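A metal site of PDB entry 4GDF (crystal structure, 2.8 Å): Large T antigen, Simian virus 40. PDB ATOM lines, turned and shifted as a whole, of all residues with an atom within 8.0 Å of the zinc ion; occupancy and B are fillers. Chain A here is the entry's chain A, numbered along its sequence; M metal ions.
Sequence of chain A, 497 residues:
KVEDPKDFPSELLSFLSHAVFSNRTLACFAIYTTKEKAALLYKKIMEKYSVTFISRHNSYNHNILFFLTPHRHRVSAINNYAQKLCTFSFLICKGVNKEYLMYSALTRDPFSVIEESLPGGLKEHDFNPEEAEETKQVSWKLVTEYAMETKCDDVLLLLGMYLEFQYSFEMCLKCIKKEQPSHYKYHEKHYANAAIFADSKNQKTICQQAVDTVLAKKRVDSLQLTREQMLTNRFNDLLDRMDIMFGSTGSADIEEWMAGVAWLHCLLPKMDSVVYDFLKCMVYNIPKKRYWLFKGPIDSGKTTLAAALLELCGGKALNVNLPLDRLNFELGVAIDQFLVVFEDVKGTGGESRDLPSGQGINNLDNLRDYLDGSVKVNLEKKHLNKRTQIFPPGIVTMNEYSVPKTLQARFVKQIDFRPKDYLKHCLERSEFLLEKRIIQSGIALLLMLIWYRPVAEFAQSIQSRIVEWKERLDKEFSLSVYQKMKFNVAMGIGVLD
SG of Cys 172 lies close to N of Lys 174. A ring nitrogen (NE2) of His 187 is in hydrogen-bond range of the backbone carbonyl oxygen (O) of Tyr 167 (2.6 Å). NE2 of His 187 is in hydrogen-bond range of O of Phe 165, 3.0 Å away. A ring nitrogen (ND1) of His 183 lies within hydrogen-bond range of the side-chain carboxylate of Glu 164, at 3.2 Å. O of Cys 175 lies close to NZ of Lys 178 (3.2 Å).
Within 4 Å of the zinc ion: Cys 172, Cys 175, His 183 and His 187.
The zinc ion is bound by the side-chain sulfur (SG) of Cys 172 (2.3 Å), the side-chain sulfur (SG) of Cys 175 (2.4 Å), a ring nitrogen (ND1) of His 187 (2.4 Å) and a ring nitrogen (NE2) of His 183 (2.5 Å). The zinc ion has four donor atoms within binding distance.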
ATOM      1  N   GLU A 164     -15.126  19.147 -30.655  1.00  0.00           N
ATOM      2  CA  GLU A 164     -14.672  18.195 -29.660  1.00  0.00           C
ATOM      3  C   GLU A 164     -13.216  17.839 -29.929  1.00  0.00           C
ATOM      4  O   GLU A 164     -12.437  17.667 -29.008  1.00  0.00           O
ATOM      5  CB  GLU A 164     -15.521  16.922 -29.696  1.00  0.00           C
ATOM      6  CG  GLU A 164     -16.862  17.011 -28.982  1.00  0.00           C
ATOM      7  CD  GLU A 164     -17.663  15.736 -29.132  1.00  0.00           C
ATOM      8  OE1 GLU A 164     -18.677  15.561 -28.427  1.00  0.00           O
ATOM      9  OE2 GLU A 164     -17.284  14.891 -29.980  1.00  0.00           O
ATOM     10  N   PHE A 165     -12.831  17.744 -31.192  1.00  0.00           N
ATOM     11  CA  PHE A 165     -11.459  17.418 -31.505  1.00  0.00           C
ATOM     12  C   PHE A 165     -10.485  18.526 -31.089  1.00  0.00           C
ATOM     13  O   PHE A 165      -9.283  18.327 -31.128  1.00  0.00           O
ATOM     14  CB  PHE A 165     -11.298  17.156 -32.993  1.00  0.00           C
ATOM     15  CG  PHE A 165     -12.257  16.151 -33.540  1.00  0.00           C
ATOM     16  CD1 PHE A 165     -12.528  14.984 -32.832  1.00  0.00           C
ATOM     17  CD2 PHE A 165     -12.840  16.333 -34.780  1.00  0.00           C
ATOM     18  CE1 PHE A 165     -13.361  14.023 -33.364  1.00  0.00           C
ATOM     19  CE2 PHE A 165     -13.678  15.363 -35.321  1.00  0.00           C
ATOM     20  CZ  PHE A 165     -13.945  14.202 -34.620  1.00  0.00           C
ATOM     21  N   GLN A 166     -10.985  19.688 -30.691  1.00  0.00           N
ATOM     22  CA  GLN A 166     -10.058  20.754 -30.358  1.00  0.00           C
ATOM     23  C   GLN A 166      -9.149  20.400 -29.231  1.00  0.00           C
ATOM     24  O   GLN A 166      -8.027  20.870 -29.177  1.00  0.00           O
ATOM     25  CB  GLN A 166     -10.793  22.025 -30.015  1.00  0.00           C
ATOM     26  CG  GLN A 166     -11.167  22.194 -28.580  1.00  0.00           C
ATOM     27  CD  GLN A 166     -11.816  23.536 -28.356  1.00  0.00           C
ATOM     28  OE1 GLN A 166     -12.940  23.757 -28.794  1.00  0.00           O
ATOM     29  NE2 GLN A 166     -11.099  24.457 -27.722  1.00  0.00           N
ATOM     30  N   TYR A 167      -9.623  19.558 -28.325  1.00  0.00           N
ATOM     31  CA  TYR A 167      -8.862  19.171 -27.160  1.00  0.00           C
ATOM     32  C   TYR A 167      -7.804  18.087 -27.405  1.00  0.00           C
ATOM     33  O   TYR A 167      -7.925  17.272 -28.320  1.00  0.00           O
ATOM     34  CB  TYR A 167      -9.829  18.726 -26.072  1.00  0.00           C
ATOM     35  CG  TYR A 167     -10.917  19.735 -25.833  1.00  0.00           C
ATOM     36  CD1 TYR A 167     -10.620  21.007 -25.370  1.00  0.00           C
ATOM     37  CD2 TYR A 167     -12.243  19.427 -26.103  1.00  0.00           C
ATOM     38  CE1 TYR A 167     -11.614  21.961 -25.170  1.00  0.00           C
ATOM     39  CE2 TYR A 167     -13.254  20.364 -25.911  1.00  0.00           C
ATOM     40  CZ  TYR A 167     -12.923  21.625 -25.441  1.00  0.00           C
ATOM     41  OH  TYR A 167     -13.909  22.562 -25.250  1.00  0.00           O
ATOM     42  N   SER A 168      -6.785  18.103 -26.560  1.00  0.00           N
ATOM     43  CA  SER A 168      -5.681  17.146 -26.628  1.00  0.00           C
ATOM     44  C   SER A 168      -6.160  15.721 -26.795  1.00  0.00           C
ATOM     45  O   SER A 168      -7.103  15.279 -26.128  1.00  0.00           O
ATOM     46  CB  SER A 168      -4.839  17.232 -25.364  1.00  0.00           C
ATOM     47  OG  SER A 168      -5.515  16.608 -24.291  1.00  0.00           O
ATOM     48  N   PHE A 169      -5.480  15.090 -27.614  1.00  0.00           N
ATOM     49  CA  PHE A 169      -5.877  13.790 -27.889  1.00  0.00           C
ATOM     50  C   PHE A 169      -5.389  12.782 -26.894  1.00  0.00           C
ATOM     51  O   PHE A 169      -6.186  12.007 -26.351  1.00  0.00           O
ATOM     52  CB  PHE A 169      -5.392  13.501 -29.296  1.00  0.00           C
ATOM     53  CG  PHE A 169      -5.467  12.090 -29.638  1.00  0.00           C
ATOM     54  CD1 PHE A 169      -6.713  11.454 -29.733  1.00  0.00           C
ATOM     55  CD2 PHE A 169      -4.319  11.335 -29.853  1.00  0.00           C
ATOM     56  CE1 PHE A 169      -6.803  10.097 -30.026  1.00  0.00           C
ATOM     57  CE2 PHE A 169      -4.397   9.984 -30.149  1.00  0.00           C
ATOM     58  CZ  PHE A 169      -5.639   9.358 -30.234  1.00  0.00           C
ATOM     59  N   GLU A 170      -4.080  12.762 -26.658  1.00  0.00           N
ATOM     60  CA  GLU A 170      -3.481  11.767 -25.789  1.00  0.00           C
ATOM     61  C   GLU A 170      -4.288  11.452 -24.536  1.00  0.00           C
ATOM     62  O   GLU A 170      -4.596  10.275 -24.262  1.00  0.00           O
ATOM     63  CB  GLU A 170      -2.045  12.164 -25.396  1.00  0.00           C
ATOM     64  CG  GLU A 170      -1.927  13.046 -24.170  1.00  0.00           C
ATOM     65  CD  GLU A 170      -0.525  12.993 -23.575  1.00  0.00           C
ATOM     66  OE1 GLU A 170      -0.146  11.909 -23.073  1.00  0.00           O
ATOM     67  OE2 GLU A 170       0.196  14.015 -23.607  1.00  0.00           O
ATOM     68  N   MET A 171      -4.642  12.467 -23.774  1.00  0.00           N
ATOM     69  CA  MET A 171      -5.409  12.254 -22.557  1.00  0.00           C
ATOM     70  C   MET A 171      -6.865  12.709 -22.700  1.00  0.00           C
ATOM     71  O   MET A 171      -7.326  13.564 -21.952  1.00  0.00           O
ATOM     72  CB  MET A 171      -4.724  12.945 -21.385  1.00  0.00           C
ATOM     73  CG  MET A 171      -3.486  13.744 -21.764  1.00  0.00           C
ATOM     74  SD  MET A 171      -2.672  14.444 -20.303  1.00  0.00           S
ATOM     75  CE  MET A 171      -3.953  15.564 -19.690  1.00  0.00           C
ATOM     76  N   CYS A 172      -7.547  12.126 -23.678  1.00  0.00           N
ATOM     77  CA  CYS A 172      -8.953  12.409 -23.986  1.00  0.00           C
ATOM     78  C   CYS A 172      -9.810  11.256 -23.468  1.00  0.00           C
ATOM     79  O   CYS A 172      -9.816  10.172 -24.051  1.00  0.00           O
ATOM     80  CB  CYS A 172      -9.128  12.553 -25.507  1.00  0.00           C
ATOM     81  SG  CYS A 172     -10.823  12.637 -26.138  1.00  0.00           S
ATOM     82  N   LEU A 173     -10.539  11.481 -22.379  1.00  0.00           N
ATOM     83  CA  LEU A 173     -11.379  10.429 -21.802  1.00  0.00           C
ATOM     84  C   LEU A 173     -12.363   9.877 -22.820  1.00  0.00           C
ATOM     85  O   LEU A 173     -12.696   8.696 -22.793  1.00  0.00           O
ATOM     86  CB  LEU A 173     -12.142  10.941 -20.585  1.00  0.00           C
ATOM     87  CG  LEU A 173     -11.316  11.254 -19.342  1.00  0.00           C
ATOM     88  CD1 LEU A 173     -10.414  12.468 -19.585  1.00  0.00           C
ATOM     89  CD2 LEU A 173     -12.272  11.541 -18.191  1.00  0.00           C
ATOM     90  N   LYS A 174     -12.837  10.744 -23.701  1.00  0.00           N
ATOM     91  CA  LYS A 174     -13.789  10.332 -24.716  1.00  0.00           C
ATOM     92  C   LYS A 174     -13.207   9.322 -25.690  1.00  0.00           C
ATOM     93  O   LYS A 174     -13.909   8.436 -26.168  1.00  0.00           O
ATOM     94  CB  LYS A 174     -14.316  11.542 -25.476  1.00  0.00           C
ATOM     95  CG  LYS A 174     -15.101  12.514 -24.603  1.00  0.00           C
ATOM     96  CD  LYS A 174     -15.746  13.580 -25.437  1.00  0.00           C
ATOM     97  CE  LYS A 174     -16.556  14.520 -24.574  1.00  0.00           C
ATOM     98  NZ  LYS A 174     -17.127  15.623 -25.384  1.00  0.00           N
ATOM     99  N   CYS A 175     -11.917   9.454 -25.984  1.00  0.00           N
ATOM    100  CA  CYS A 175     -11.238   8.535 -26.893  1.00  0.00           C
ATOM    101  C   CYS A 175     -10.857   7.258 -26.148  1.00  0.00           C
ATOM    102  O   CYS A 175     -10.911   6.162 -26.708  1.00  0.00           O
ATOM    103  CB  CYS A 175     -10.004   9.202 -27.515  1.00  0.00           C
ATOM    104  SG  CYS A 175     -10.293  10.001 -29.135  1.00  0.00           S
ATOM    105  N   ILE A 176     -10.474   7.398 -24.888  1.00  0.00           N
ATOM    106  CA  ILE A 176     -10.090   6.259 -24.073  1.00  0.00           C
ATOM    107  C   ILE A 176     -11.290   5.343 -23.835  1.00  0.00           C
ATOM    108  O   ILE A 176     -11.270   4.173 -24.187  1.00  0.00           O
ATOM    109  CB  ILE A 176      -9.555   6.717 -22.707  1.00  0.00           C
ATOM    110  CG1 ILE A 176      -8.323   7.592 -22.907  1.00  0.00           C
ATOM    111  CG2 ILE A 176      -9.211   5.507 -21.845  1.00  0.00           C
ATOM    112  CD1 ILE A 176      -7.802   8.209 -21.640  1.00  0.00           C
ATOM    113  N   LYS A 178     -13.727   5.185 -25.368  1.00  0.00           N
ATOM    114  CA  LYS A 178     -14.310   4.854 -26.672  1.00  0.00           C
ATOM    115  C   LYS A 178     -15.826   4.833 -26.660  1.00  0.00           C
ATOM    116  O   LYS A 178     -16.460   3.801 -26.919  1.00  0.00           O
ATOM    117  CB  LYS A 178     -13.761   3.516 -27.158  1.00  0.00           C
ATOM    118  CG  LYS A 178     -12.254   3.519 -27.284  1.00  0.00           C
ATOM    119  CD  LYS A 178     -11.771   2.490 -28.267  1.00  0.00           C
ATOM    120  CE  LYS A 178     -10.269   2.625 -28.482  1.00  0.00           C
ATOM    121  NZ  LYS A 178      -9.868   4.031 -28.816  1.00  0.00           N
ATOM    122  N   GLN A 180     -18.100   7.124 -28.516  1.00  0.00           N
ATOM    123  CA  GLN A 180     -18.658   7.250 -29.857  1.00  0.00           C
ATOM    124  C   GLN A 180     -17.614   6.912 -30.923  1.00  0.00           C
ATOM    125  O   GLN A 180     -16.533   7.506 -30.954  1.00  0.00           O
ATOM    126  CB  GLN A 180     -19.200   8.658 -30.074  1.00  0.00           C
ATOM    127  CG  GLN A 180     -20.514   8.950 -29.364  1.00  0.00           C
ATOM    128  CD  GLN A 180     -21.643   8.031 -29.816  1.00  0.00           C
ATOM    129  OE1 GLN A 180     -21.882   7.868 -31.012  1.00  0.00           O
ATOM    130  NE2 GLN A 180     -22.350   7.439 -28.854  1.00  0.00           N
ATOM    131  N   HIS A 183     -15.802   9.405 -33.395  1.00  0.00           N
ATOM    132  CA  HIS A 183     -15.020  10.375 -32.650  1.00  0.00           C
ATOM    133  C   HIS A 183     -13.621   9.828 -32.389  1.00  0.00           C
ATOM    134  O   HIS A 183     -12.643  10.391 -32.876  1.00  0.00           O
ATOM    135  CB  HIS A 183     -15.657  10.714 -31.318  1.00  0.00           C
ATOM    136  CG  HIS A 183     -14.840  11.640 -30.481  1.00  0.00           C
ATOM    137  ND1 HIS A 183     -14.824  13.002 -30.683  1.00  0.00           N
ATOM    138  CD2 HIS A 183     -13.953  11.395 -29.484  1.00  0.00           C
ATOM    139  CE1 HIS A 183     -13.968  13.561 -29.844  1.00  0.00           C
ATOM    140  NE2 HIS A 183     -13.425  12.607 -29.106  1.00  0.00           N
ATOM    141  N   TYR A 184     -13.523   8.746 -31.627  1.00  0.00           N
ATOM    142  CA  TYR A 184     -12.231   8.170 -31.320  1.00  0.00           C
ATOM    143  C   TYR A 184     -11.566   7.677 -32.596  1.00  0.00           C
ATOM    144  O   TYR A 184     -10.396   7.302 -32.570  1.00  0.00           O
ATOM    145  CB  TYR A 184     -12.342   7.048 -30.268  1.00  0.00           C
ATOM    146  CG  TYR A 184     -13.134   5.815 -30.694  1.00  0.00           C
ATOM    147  CD1 TYR A 184     -12.697   5.008 -31.743  1.00  0.00           C
ATOM    148  CD2 TYR A 184     -14.305   5.457 -30.031  1.00  0.00           C
ATOM    149  CE1 TYR A 184     -13.421   3.879 -32.136  1.00  0.00           C
ATOM    150  CE2 TYR A 184     -15.039   4.325 -30.405  1.00  0.00           C
ATOM    151  CZ  TYR A 184     -14.588   3.545 -31.466  1.00  0.00           C
ATOM    152  OH  TYR A 184     -15.296   2.442 -31.872  1.00  0.00           O
ATOM    153  N   LYS A 185     -12.300   7.682 -33.695  1.00  0.00           N
ATOM    154  CA  LYS A 185     -11.730   7.238 -34.965  1.00  0.00           C
ATOM    155  C   LYS A 185     -11.154   8.376 -35.793  1.00  0.00           C
ATOM    156  O   LYS A 185     -10.380   8.138 -36.721  1.00  0.00           O
ATOM    157  CB  LYS A 185     -12.771   6.522 -35.826  1.00  0.00           C
ATOM    158  CG  LYS A 185     -12.447   5.102 -36.213  1.00  0.00           C
ATOM    159  CD  LYS A 185     -13.625   4.507 -36.965  1.00  0.00           C
ATOM    160  CE  LYS A 185     -14.713   4.058 -36.007  1.00  0.00           C
ATOM    161  NZ  LYS A 185     -15.956   3.648 -36.726  1.00  0.00           N
ATOM    162  N   TYR A 186     -11.545   9.611 -35.475  1.00  0.00           N
ATOM    163  CA  TYR A 186     -11.074  10.756 -36.252  1.00  0.00           C
ATOM    164  C   TYR A 186     -10.396  11.880 -35.477  1.00  0.00           C
ATOM    165  O   TYR A 186      -9.836  12.805 -36.085  1.00  0.00           O
ATOM    166  CB  TYR A 186     -12.251  11.362 -37.038  1.00  0.00           C
ATOM    167  CG  TYR A 186     -13.014  10.371 -37.886  1.00  0.00           C
ATOM    168  CD1 TYR A 186     -13.832   9.407 -37.311  1.00  0.00           C
ATOM    169  CD2 TYR A 186     -12.917  10.410 -39.278  1.00  0.00           C
ATOM    170  CE1 TYR A 186     -14.532   8.498 -38.092  1.00  0.00           C
ATOM    171  CE2 TYR A 186     -13.622   9.505 -40.071  1.00  0.00           C
ATOM    172  CZ  TYR A 186     -14.423   8.548 -39.469  1.00  0.00           C
ATOM    173  OH  TYR A 186     -15.119   7.648 -40.239  1.00  0.00           O
ATOM    174  N   HIS A 187     -10.439  11.812 -34.163  1.00  0.00           N
ATOM    175  CA  HIS A 187      -9.835  12.863 -33.345  1.00  0.00           C
ATOM    176  C   HIS A 187      -8.357  13.069 -33.598  1.00  0.00           C
ATOM    177  O   HIS A 187      -7.962  14.118 -34.108  1.00  0.00           O
ATOM    178  CB  HIS A 187     -10.070  12.587 -31.853  1.00  0.00           C
ATOM    179  CG  HIS A 187      -9.699  13.736 -30.976  1.00  0.00           C
ATOM    180  ND1 HIS A 187     -10.017  13.772 -29.632  1.00  0.00           N
ATOM    181  CD2 HIS A 187      -9.026  14.880 -31.235  1.00  0.00           C
ATOM    182  CE1 HIS A 187      -9.565  14.890 -29.106  1.00  0.00           C
ATOM    183  NE2 HIS A 187      -8.957  15.584 -30.050  1.00  0.00           N
ATOM    184  N   GLU A 188      -7.534  12.092 -33.247  1.00  0.00           N
ATOM    185  CA  GLU A 188      -6.087  12.215 -33.444  1.00  0.00           C
ATOM    186  C   GLU A 188      -5.761  12.833 -34.814  1.00  0.00           C
ATOM    187  O   GLU A 188      -4.947  13.746 -34.928  1.00  0.00           O
ATOM    188  CB  GLU A 188      -5.402  10.858 -33.281  1.00  0.00           C
ATOM    189  CG  GLU A 188      -3.892  10.872 -33.492  1.00  0.00           C
ATOM    190  CD  GLU A 188      -3.234   9.552 -33.123  1.00  0.00           C
ATOM    191  OE1 GLU A 188      -3.725   8.480 -33.562  1.00  0.00           O
ATOM    192  OE2 GLU A 188      -2.217   9.579 -32.392  1.00  0.00           O
HETATM  193 ZN    ZN M   1     -11.120  12.079 -28.298  1.00  0.00          ZN
